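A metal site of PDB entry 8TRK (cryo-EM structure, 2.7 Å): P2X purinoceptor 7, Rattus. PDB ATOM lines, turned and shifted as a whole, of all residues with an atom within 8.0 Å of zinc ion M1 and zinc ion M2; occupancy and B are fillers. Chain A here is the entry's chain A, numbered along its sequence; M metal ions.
Of the 28 residues printed, 4 come within 4 Å of zinc ion M1.
Zinc ion M1 is bound by the side-chain sulfur (SG) of Cys 572 (2.3 Å), the side-chain sulfur (SG) of Cys 499 (2.3 Å), the side-chain sulfur (SG) of Cys 506 (2.3 Å) and the side-chain sulfur (SG) of Cys 479 (2.3 Å).
The side-chain sulfur (SG) of Cys 479 binds zinc ion M2, at 2.3 Å.
The side-chain sulfur (SG) of Cys 482 binds zinc ion M2.
Zinc ion M2 is bound by SG of Cys 498 (2.3 Å).
SG of Cys 477 binds zinc ion M2, at 2.3 Å.
N of Gly 480 touches zinc ion M2 (3.9 Å).
Along chain A the residues within 4 Å of zinc ion M2 span positions 477 to 498.
The nearest printed residue that does not touch zinc ion M2 is Gln 478 (4.1 Å).
OD1 of Asn 481 sits close to O of Cys 479 (2.8 Å).
The side-chain sulfur (SG) of Cys 482 lies close to the backbone NH (N) of Cys 572.
N of Gln 478 lies close to SG of Cys 498.
The backbone NH (N) of Cys 498 sits at hydrogen-bond distance from the side-chain amide oxygen (OE1) of Gln 422, 2.9 Å away.
O of Cys 499 is in hydrogen-bond range of N of Val 404.
OG1 of Thr 508 sits close to SG of Cys 506 (2.8 Å).
The backbone NH of Gly 480 sits close to the side-chain sulfur of Cys 477, 2.9 Å away.
N of Asn 481 lies close to SG of Cys 477, at 3.7 Å.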
ATOM      1  N   VAL A 404      31.895 -13.182  18.242  1.00  0.00           N
ATOM      2  CA  VAL A 404      32.057 -11.776  17.906  1.00  0.00           C
ATOM      3  C   VAL A 404      33.354 -11.211  18.449  1.00  0.00           C
ATOM      4  O   VAL A 404      33.793 -10.140  18.016  1.00  0.00           O
ATOM      5  CB  VAL A 404      30.860 -10.973  18.444  1.00  0.00           C
ATOM      6  CG1 VAL A 404      30.880 -10.923  19.939  1.00  0.00           C
ATOM      7  CG2 VAL A 404      30.849  -9.585  17.856  1.00  0.00           C
ATOM      8  N   GLN A 422      29.780 -24.767  22.829  1.00  0.00           N
ATOM      9  CA  GLN A 422      30.683 -23.685  23.201  1.00  0.00           C
ATOM     10  C   GLN A 422      32.081 -24.208  23.515  1.00  0.00           C
ATOM     11  O   GLN A 422      33.069 -23.547  23.187  1.00  0.00           O
ATOM     12  CB  GLN A 422      30.106 -22.945  24.397  1.00  0.00           C
ATOM     13  CG  GLN A 422      30.916 -21.758  24.870  1.00  0.00           C
ATOM     14  CD  GLN A 422      30.754 -20.548  24.006  1.00  0.00           C
ATOM     15  OE1 GLN A 422      30.096 -20.589  22.967  1.00  0.00           O
ATOM     16  NE2 GLN A 422      31.347 -19.454  24.430  1.00  0.00           N
ATOM     17  N   SER A 473      23.074 -16.536  34.631  1.00  0.00           N
ATOM     18  CA  SER A 473      23.286 -17.060  33.297  1.00  0.00           C
ATOM     19  C   SER A 473      23.967 -18.418  33.356  1.00  0.00           C
ATOM     20  O   SER A 473      24.573 -18.778  34.365  1.00  0.00           O
ATOM     21  CB  SER A 473      24.127 -16.085  32.479  1.00  0.00           C
ATOM     22  OG  SER A 473      25.485 -16.121  32.868  1.00  0.00           O
ATOM     23  N   PRO A 474      23.885 -19.198  32.278  1.00  0.00           N
ATOM     24  CA  PRO A 474      24.512 -20.518  32.282  1.00  0.00           C
ATOM     25  C   PRO A 474      26.017 -20.437  32.473  1.00  0.00           C
ATOM     26  O   PRO A 474      26.631 -19.366  32.431  1.00  0.00           O
ATOM     27  CB  PRO A 474      24.152 -21.081  30.898  1.00  0.00           C
ATOM     28  CG  PRO A 474      22.989 -20.312  30.454  1.00  0.00           C
ATOM     29  CD  PRO A 474      23.155 -18.952  31.028  1.00  0.00           C
ATOM     30  N   TRP A 476      28.242 -21.709  30.481  1.00  0.00           N
ATOM     31  CA  TRP A 476      28.915 -21.585  29.196  1.00  0.00           C
ATOM     32  C   TRP A 476      28.673 -20.231  28.536  1.00  0.00           C
ATOM     33  O   TRP A 476      29.208 -19.985  27.448  1.00  0.00           O
ATOM     34  CB  TRP A 476      28.486 -22.704  28.249  1.00  0.00           C
ATOM     35  CG  TRP A 476      27.002 -22.935  28.213  1.00  0.00           C
ATOM     36  CD1 TRP A 476      26.311 -23.921  28.864  1.00  0.00           C
ATOM     37  CD2 TRP A 476      26.028 -22.192  27.474  1.00  0.00           C
ATOM     38  NE1 TRP A 476      24.977 -23.828  28.586  1.00  0.00           N
ATOM     39  CE2 TRP A 476      24.775 -22.763  27.734  1.00  0.00           C
ATOM     40  CE3 TRP A 476      26.101 -21.078  26.630  1.00  0.00           C
ATOM     41  CZ2 TRP A 476      23.604 -22.272  27.177  1.00  0.00           C
ATOM     42  CZ3 TRP A 476      24.937 -20.604  26.086  1.00  0.00           C
ATOM     43  CH2 TRP A 476      23.703 -21.195  26.356  1.00  0.00           C
ATOM     44  N   CYS A 477      27.883 -19.354  29.145  1.00  0.00           N
ATOM     45  CA  CYS A 477      27.545 -18.075  28.565  1.00  0.00           C
ATOM     46  C   CYS A 477      28.447 -16.988  29.124  1.00  0.00           C
ATOM     47  O   CYS A 477      28.527 -16.821  30.347  1.00  0.00           O
ATOM     48  CB  CYS A 477      26.079 -17.721  28.817  1.00  0.00           C
ATOM     49  SG  CYS A 477      25.661 -16.021  28.439  1.00  0.00           S
ATOM     50  N   GLN A 478      29.097 -16.248  28.230  1.00  0.00           N
ATOM     51  CA  GLN A 478      29.929 -15.119  28.600  1.00  0.00           C
ATOM     52  C   GLN A 478      29.242 -13.780  28.368  1.00  0.00           C
ATOM     53  O   GLN A 478      29.714 -12.766  28.894  1.00  0.00           O
ATOM     54  CB  GLN A 478      31.233 -15.155  27.813  1.00  0.00           C
ATOM     55  CG  GLN A 478      31.835 -16.535  27.623  1.00  0.00           C
ATOM     56  CD  GLN A 478      32.438 -17.092  28.900  1.00  0.00           C
ATOM     57  OE1 GLN A 478      32.082 -16.672  30.000  1.00  0.00           O
ATOM     58  NE2 GLN A 478      33.341 -18.036  28.742  1.00  0.00           N
ATOM     59  N   CYS A 479      28.151 -13.751  27.609  1.00  0.00           N
ATOM     60  CA  CYS A 479      27.445 -12.509  27.335  1.00  0.00           C
ATOM     61  C   CYS A 479      26.367 -12.210  28.371  1.00  0.00           C
ATOM     62  O   CYS A 479      25.938 -11.060  28.464  1.00  0.00           O
ATOM     63  CB  CYS A 479      26.821 -12.563  25.939  1.00  0.00           C
ATOM     64  SG  CYS A 479      25.238 -13.434  25.785  1.00  0.00           S
ATOM     65  N   GLY A 480      25.936 -13.208  29.135  1.00  0.00           N
ATOM     66  CA  GLY A 480      24.958 -13.003  30.168  1.00  0.00           C
ATOM     67  C   GLY A 480      23.530 -12.967  29.681  1.00  0.00           C
ATOM     68  O   GLY A 480      22.610 -12.816  30.494  1.00  0.00           O
ATOM     69  N   ASN A 481      23.313 -13.126  28.380  1.00  0.00           N
ATOM     70  CA  ASN A 481      21.992 -13.003  27.784  1.00  0.00           C
ATOM     71  C   ASN A 481      21.501 -14.312  27.182  1.00  0.00           C
ATOM     72  O   ASN A 481      20.431 -14.336  26.553  1.00  0.00           O
ATOM     73  CB  ASN A 481      22.021 -11.902  26.716  1.00  0.00           C
ATOM     74  CG  ASN A 481      22.243 -10.548  27.317  1.00  0.00           C
ATOM     75  OD1 ASN A 481      23.361 -10.226  27.698  1.00  0.00           O
ATOM     76  ND2 ASN A 481      21.204  -9.755  27.410  1.00  0.00           N
ATOM     77  N   CYS A 482      22.252 -15.393  27.338  1.00  0.00           N
ATOM     78  CA  CYS A 482      21.848 -16.688  26.831  1.00  0.00           C
ATOM     79  C   CYS A 482      20.982 -17.411  27.854  1.00  0.00           C
ATOM     80  O   CYS A 482      21.028 -17.129  29.053  1.00  0.00           O
ATOM     81  CB  CYS A 482      23.075 -17.529  26.500  1.00  0.00           C
ATOM     82  SG  CYS A 482      24.034 -16.975  25.084  1.00  0.00           S
ATOM     83  N   LEU A 483      20.195 -18.355  27.368  1.00  0.00           N
ATOM     84  CA  LEU A 483      19.226 -19.069  28.172  1.00  0.00           C
ATOM     85  C   LEU A 483      19.408 -20.569  28.013  1.00  0.00           C
ATOM     86  O   LEU A 483      19.939 -21.027  26.994  1.00  0.00           O
ATOM     87  CB  LEU A 483      17.795 -18.690  27.790  1.00  0.00           C
ATOM     88  CG  LEU A 483      17.504 -17.192  27.678  1.00  0.00           C
ATOM     89  CD1 LEU A 483      16.095 -16.977  27.188  1.00  0.00           C
ATOM     90  CD2 LEU A 483      17.738 -16.502  29.006  1.00  0.00           C
ATOM     91  N   LEU A 497      25.480 -22.573  22.983  1.00  0.00           N
ATOM     92  CA  LEU A 497      26.490 -21.733  22.352  1.00  0.00           C
ATOM     93  C   LEU A 497      26.253 -20.284  22.706  1.00  0.00           C
ATOM     94  O   LEU A 497      25.116 -19.826  22.810  1.00  0.00           O
ATOM     95  CB  LEU A 497      26.470 -21.927  20.844  1.00  0.00           C
ATOM     96  CG  LEU A 497      27.511 -21.218  19.996  1.00  0.00           C
ATOM     97  CD1 LEU A 497      28.875 -21.834  20.178  1.00  0.00           C
ATOM     98  CD2 LEU A 497      27.082 -21.297  18.572  1.00  0.00           C
ATOM     99  N   CYS A 498      27.346 -19.546  22.878  1.00  0.00           N
ATOM    100  CA  CYS A 498      27.308 -18.118  23.182  1.00  0.00           C
ATOM    101  C   CYS A 498      27.922 -17.332  22.040  1.00  0.00           C
ATOM    102  O   CYS A 498      28.679 -17.859  21.208  1.00  0.00           O
ATOM    103  CB  CYS A 498      28.052 -17.795  24.480  1.00  0.00           C
ATOM    104  SG  CYS A 498      27.718 -16.157  25.147  1.00  0.00           S
ATOM    105  N   CYS A 499      27.598 -16.043  22.008  1.00  0.00           N
ATOM    106  CA  CYS A 499      28.082 -15.132  20.982  1.00  0.00           C
ATOM    107  C   CYS A 499      29.577 -14.860  21.076  1.00  0.00           C
ATOM    108  O   CYS A 499      30.139 -14.351  20.102  1.00  0.00           O
ATOM    109  CB  CYS A 499      27.309 -13.818  21.066  1.00  0.00           C
ATOM    110  SG  CYS A 499      27.354 -13.011  22.672  1.00  0.00           S
ATOM    111  N   ARG A 500      30.222 -15.191  22.191  1.00  0.00           N
ATOM    112  CA  ARG A 500      31.617 -14.844  22.381  1.00  0.00           C
ATOM    113  C   ARG A 500      32.275 -15.873  23.290  1.00  0.00           C
ATOM    114  O   ARG A 500      31.602 -16.605  24.016  1.00  0.00           O
ATOM    115  CB  ARG A 500      31.761 -13.439  22.947  1.00  0.00           C
ATOM    116  CG  ARG A 500      30.916 -13.180  24.175  1.00  0.00           C
ATOM    117  CD  ARG A 500      30.869 -11.711  24.469  1.00  0.00           C
ATOM    118  NE  ARG A 500      32.167 -11.085  24.237  1.00  0.00           N
ATOM    119  CZ  ARG A 500      32.339  -9.836  23.834  1.00  0.00           C
ATOM    120  NH1 ARG A 500      31.300  -9.050  23.610  1.00  0.00           N
ATOM    121  NH2 ARG A 500      33.564  -9.379  23.660  1.00  0.00           N
ATOM    122  N   GLY A 504      31.823 -10.147  27.981  1.00  0.00           N
ATOM    123  CA  GLY A 504      31.705  -8.887  27.304  1.00  0.00           C
ATOM    124  C   GLY A 504      30.261  -8.603  26.949  1.00  0.00           C
ATOM    125  O   GLY A 504      29.349  -9.277  27.425  1.00  0.00           O
ATOM    126  N   GLN A 505      30.074  -7.592  26.111  1.00  0.00           N
ATOM    127  CA  GLN A 505      28.737  -7.216  25.685  1.00  0.00           C
ATOM    128  C   GLN A 505      28.227  -8.176  24.614  1.00  0.00           C
ATOM    129  O   GLN A 505      28.984  -8.620  23.737  1.00  0.00           O
ATOM    130  CB  GLN A 505      28.714  -5.790  25.154  1.00  0.00           C
ATOM    131  CG  GLN A 505      29.757  -5.484  24.098  1.00  0.00           C
ATOM    132  CD  GLN A 505      29.390  -4.285  23.242  1.00  0.00           C
ATOM    133  OE1 GLN A 505      28.224  -4.079  22.926  1.00  0.00           O
ATOM    134  NE2 GLN A 505      30.397  -3.505  22.855  1.00  0.00           N
ATOM    135  N   CYS A 506      26.957  -8.512  24.699  1.00  0.00           N
ATOM    136  CA  CYS A 506      26.345  -9.414  23.728  1.00  0.00           C
ATOM    137  C   CYS A 506      26.260  -8.742  22.364  1.00  0.00           C
ATOM    138  O   CYS A 506      26.112  -7.523  22.243  1.00  0.00           O
ATOM    139  CB  CYS A 506      24.960  -9.833  24.189  1.00  0.00           C
ATOM    140  SG  CYS A 506      24.137 -11.002  23.103  1.00  0.00           S
ATOM    141  N   ILE A 507      26.344  -9.564  21.318  1.00  0.00           N
ATOM    142  CA  ILE A 507      26.177  -9.065  19.964  1.00  0.00           C
ATOM    143  C   ILE A 507      24.796  -8.454  19.769  1.00  0.00           C
ATOM    144  O   ILE A 507      24.611  -7.560  18.945  1.00  0.00           O
ATOM    145  CB  ILE A 507      26.435 -10.201  18.957  1.00  0.00           C
ATOM    146  CG1 ILE A 507      26.585  -9.639  17.547  1.00  0.00           C
ATOM    147  CG2 ILE A 507      25.308 -11.203  18.994  1.00  0.00           C
ATOM    148  CD1 ILE A 507      27.356 -10.524  16.646  1.00  0.00           C
ATOM    149  N   THR A 508      23.809  -8.942  20.520  1.00  0.00           N
ATOM    150  CA  THR A 508      22.454  -8.405  20.431  1.00  0.00           C
ATOM    151  C   THR A 508      22.394  -6.924  20.801  1.00  0.00           C
ATOM    152  O   THR A 508      21.442  -6.245  20.407  1.00  0.00           O
ATOM    153  CB  THR A 508      21.525  -9.191  21.330  1.00  0.00           C
ATOM    154  OG1 THR A 508      22.058  -9.236  22.652  1.00  0.00           O
ATOM    155  CG2 THR A 508      21.387 -10.594  20.833  1.00  0.00           C
ATOM    156  N   THR A 509      23.373  -6.428  21.559  1.00  0.00           N
ATOM    157  CA  THR A 509      23.328  -5.048  21.998  1.00  0.00           C
ATOM    158  C   THR A 509      23.629  -4.077  20.870  1.00  0.00           C
ATOM    159  O   THR A 509      23.242  -2.908  20.935  1.00  0.00           O
ATOM    160  CB  THR A 509      24.318  -4.831  23.148  1.00  0.00           C
ATOM    161  OG1 THR A 509      25.650  -5.086  22.696  1.00  0.00           O
ATOM    162  CG2 THR A 509      23.988  -5.778  24.292  1.00  0.00           C
ATOM    163  N   TYR A 553      20.912 -13.467  10.337  1.00  0.00           N
ATOM    164  CA  TYR A 553      22.069 -13.551  11.233  1.00  0.00           C
ATOM    165  C   TYR A 553      23.148 -14.447  10.627  1.00  0.00           C
ATOM    166  O   TYR A 553      24.329 -14.102  10.647  1.00  0.00           O
ATOM    167  CB  TYR A 553      21.659 -14.067  12.608  1.00  0.00           C
ATOM    168  CG  TYR A 553      22.837 -14.226  13.540  1.00  0.00           C
ATOM    169  CD1 TYR A 553      23.261 -13.173  14.323  1.00  0.00           C
ATOM    170  CD2 TYR A 553      23.538 -15.415  13.614  1.00  0.00           C
ATOM    171  CE1 TYR A 553      24.340 -13.303  15.163  1.00  0.00           C
ATOM    172  CE2 TYR A 553      24.609 -15.549  14.453  1.00  0.00           C
ATOM    173  CZ  TYR A 553      25.010 -14.488  15.219  1.00  0.00           C
ATOM    174  OH  TYR A 553      26.091 -14.637  16.048  1.00  0.00           O
ATOM    175  N   PRO A 570      23.811 -18.514  18.342  1.00  0.00           N
ATOM    176  CA  PRO A 570      23.915 -18.559  19.800  1.00  0.00           C
ATOM    177  C   PRO A 570      22.550 -18.528  20.461  1.00  0.00           C
ATOM    178  O   PRO A 570      21.542 -18.150  19.873  1.00  0.00           O
ATOM    179  CB  PRO A 570      24.721 -17.305  20.139  1.00  0.00           C
ATOM    180  CG  PRO A 570      25.370 -16.915  18.883  1.00  0.00           C
ATOM    181  CD  PRO A 570      24.466 -17.321  17.802  1.00  0.00           C
ATOM    182  N   SER A 571      22.536 -18.935  21.731  1.00  0.00           N
ATOM    183  CA  SER A 571      21.291 -18.911  22.494  1.00  0.00           C
ATOM    184  C   SER A 571      20.770 -17.496  22.653  1.00  0.00           C
ATOM    185  O   SER A 571      19.558 -17.271  22.628  1.00  0.00           O
ATOM    186  CB  SER A 571      21.517 -19.561  23.849  1.00  0.00           C
ATOM    187  OG  SER A 571      21.422 -20.970  23.762  1.00  0.00           O
ATOM    188  N   CYS A 572      21.665 -16.520  22.814  1.00  0.00           N
ATOM    189  CA  CYS A 572      21.242 -15.137  22.981  1.00  0.00           C
ATOM    190  C   CYS A 572      20.485 -14.636  21.752  1.00  0.00           C
ATOM    191  O   CYS A 572      19.339 -14.183  21.854  1.00  0.00           O
ATOM    192  CB  CYS A 572      22.461 -14.272  23.263  1.00  0.00           C
ATOM    193  SG  CYS A 572      23.891 -14.550  22.213  1.00  0.00           S
ATOM    194  N   CYS A 573      21.100 -14.732  20.577  1.00  0.00           N
ATOM    195  CA  CYS A 573      20.459 -14.274  19.350  1.00  0.00           C
ATOM    196  C   CYS A 573      19.209 -15.095  19.050  1.00  0.00           C
ATOM    197  O   CYS A 573      18.163 -14.550  18.677  1.00  0.00           O
ATOM    198  CB  CYS A 573      21.441 -14.347  18.196  1.00  0.00           C
ATOM    199  SG  CYS A 573      22.968 -13.432  18.437  1.00  0.00           S
ATOM    200  N   ARG A 574      19.314 -16.421  19.204  1.00  0.00           N
ATOM    201  CA  ARG A 574      18.183 -17.300  18.932  1.00  0.00           C
ATOM    202  C   ARG A 574      16.982 -16.921  19.769  1.00  0.00           C
ATOM    203  O   ARG A 574      15.867 -16.783  19.248  1.00  0.00           O
ATOM    204  CB  ARG A 574      18.615 -18.739  19.194  1.00  0.00           C
ATOM    205  CG  ARG A 574      17.515 -19.755  19.198  1.00  0.00           C
ATOM    206  CD  ARG A 574      17.985 -21.058  19.766  1.00  0.00           C
ATOM    207  NE  ARG A 574      19.253 -21.472  19.170  1.00  0.00           N
ATOM    208  CZ  ARG A 574      19.363 -21.989  17.951  1.00  0.00           C
ATOM    209  NH1 ARG A 574      18.298 -22.135  17.194  1.00  0.00           N
ATOM    210  NH2 ARG A 574      20.551 -22.344  17.499  1.00  0.00           N
HETATM  211 ZN    ZN M   1      25.164 -13.065  23.471  1.00  0.00          ZN
HETATM  212 ZN    ZN M   2      25.662 -15.682  26.125  1.00  0.00          ZN
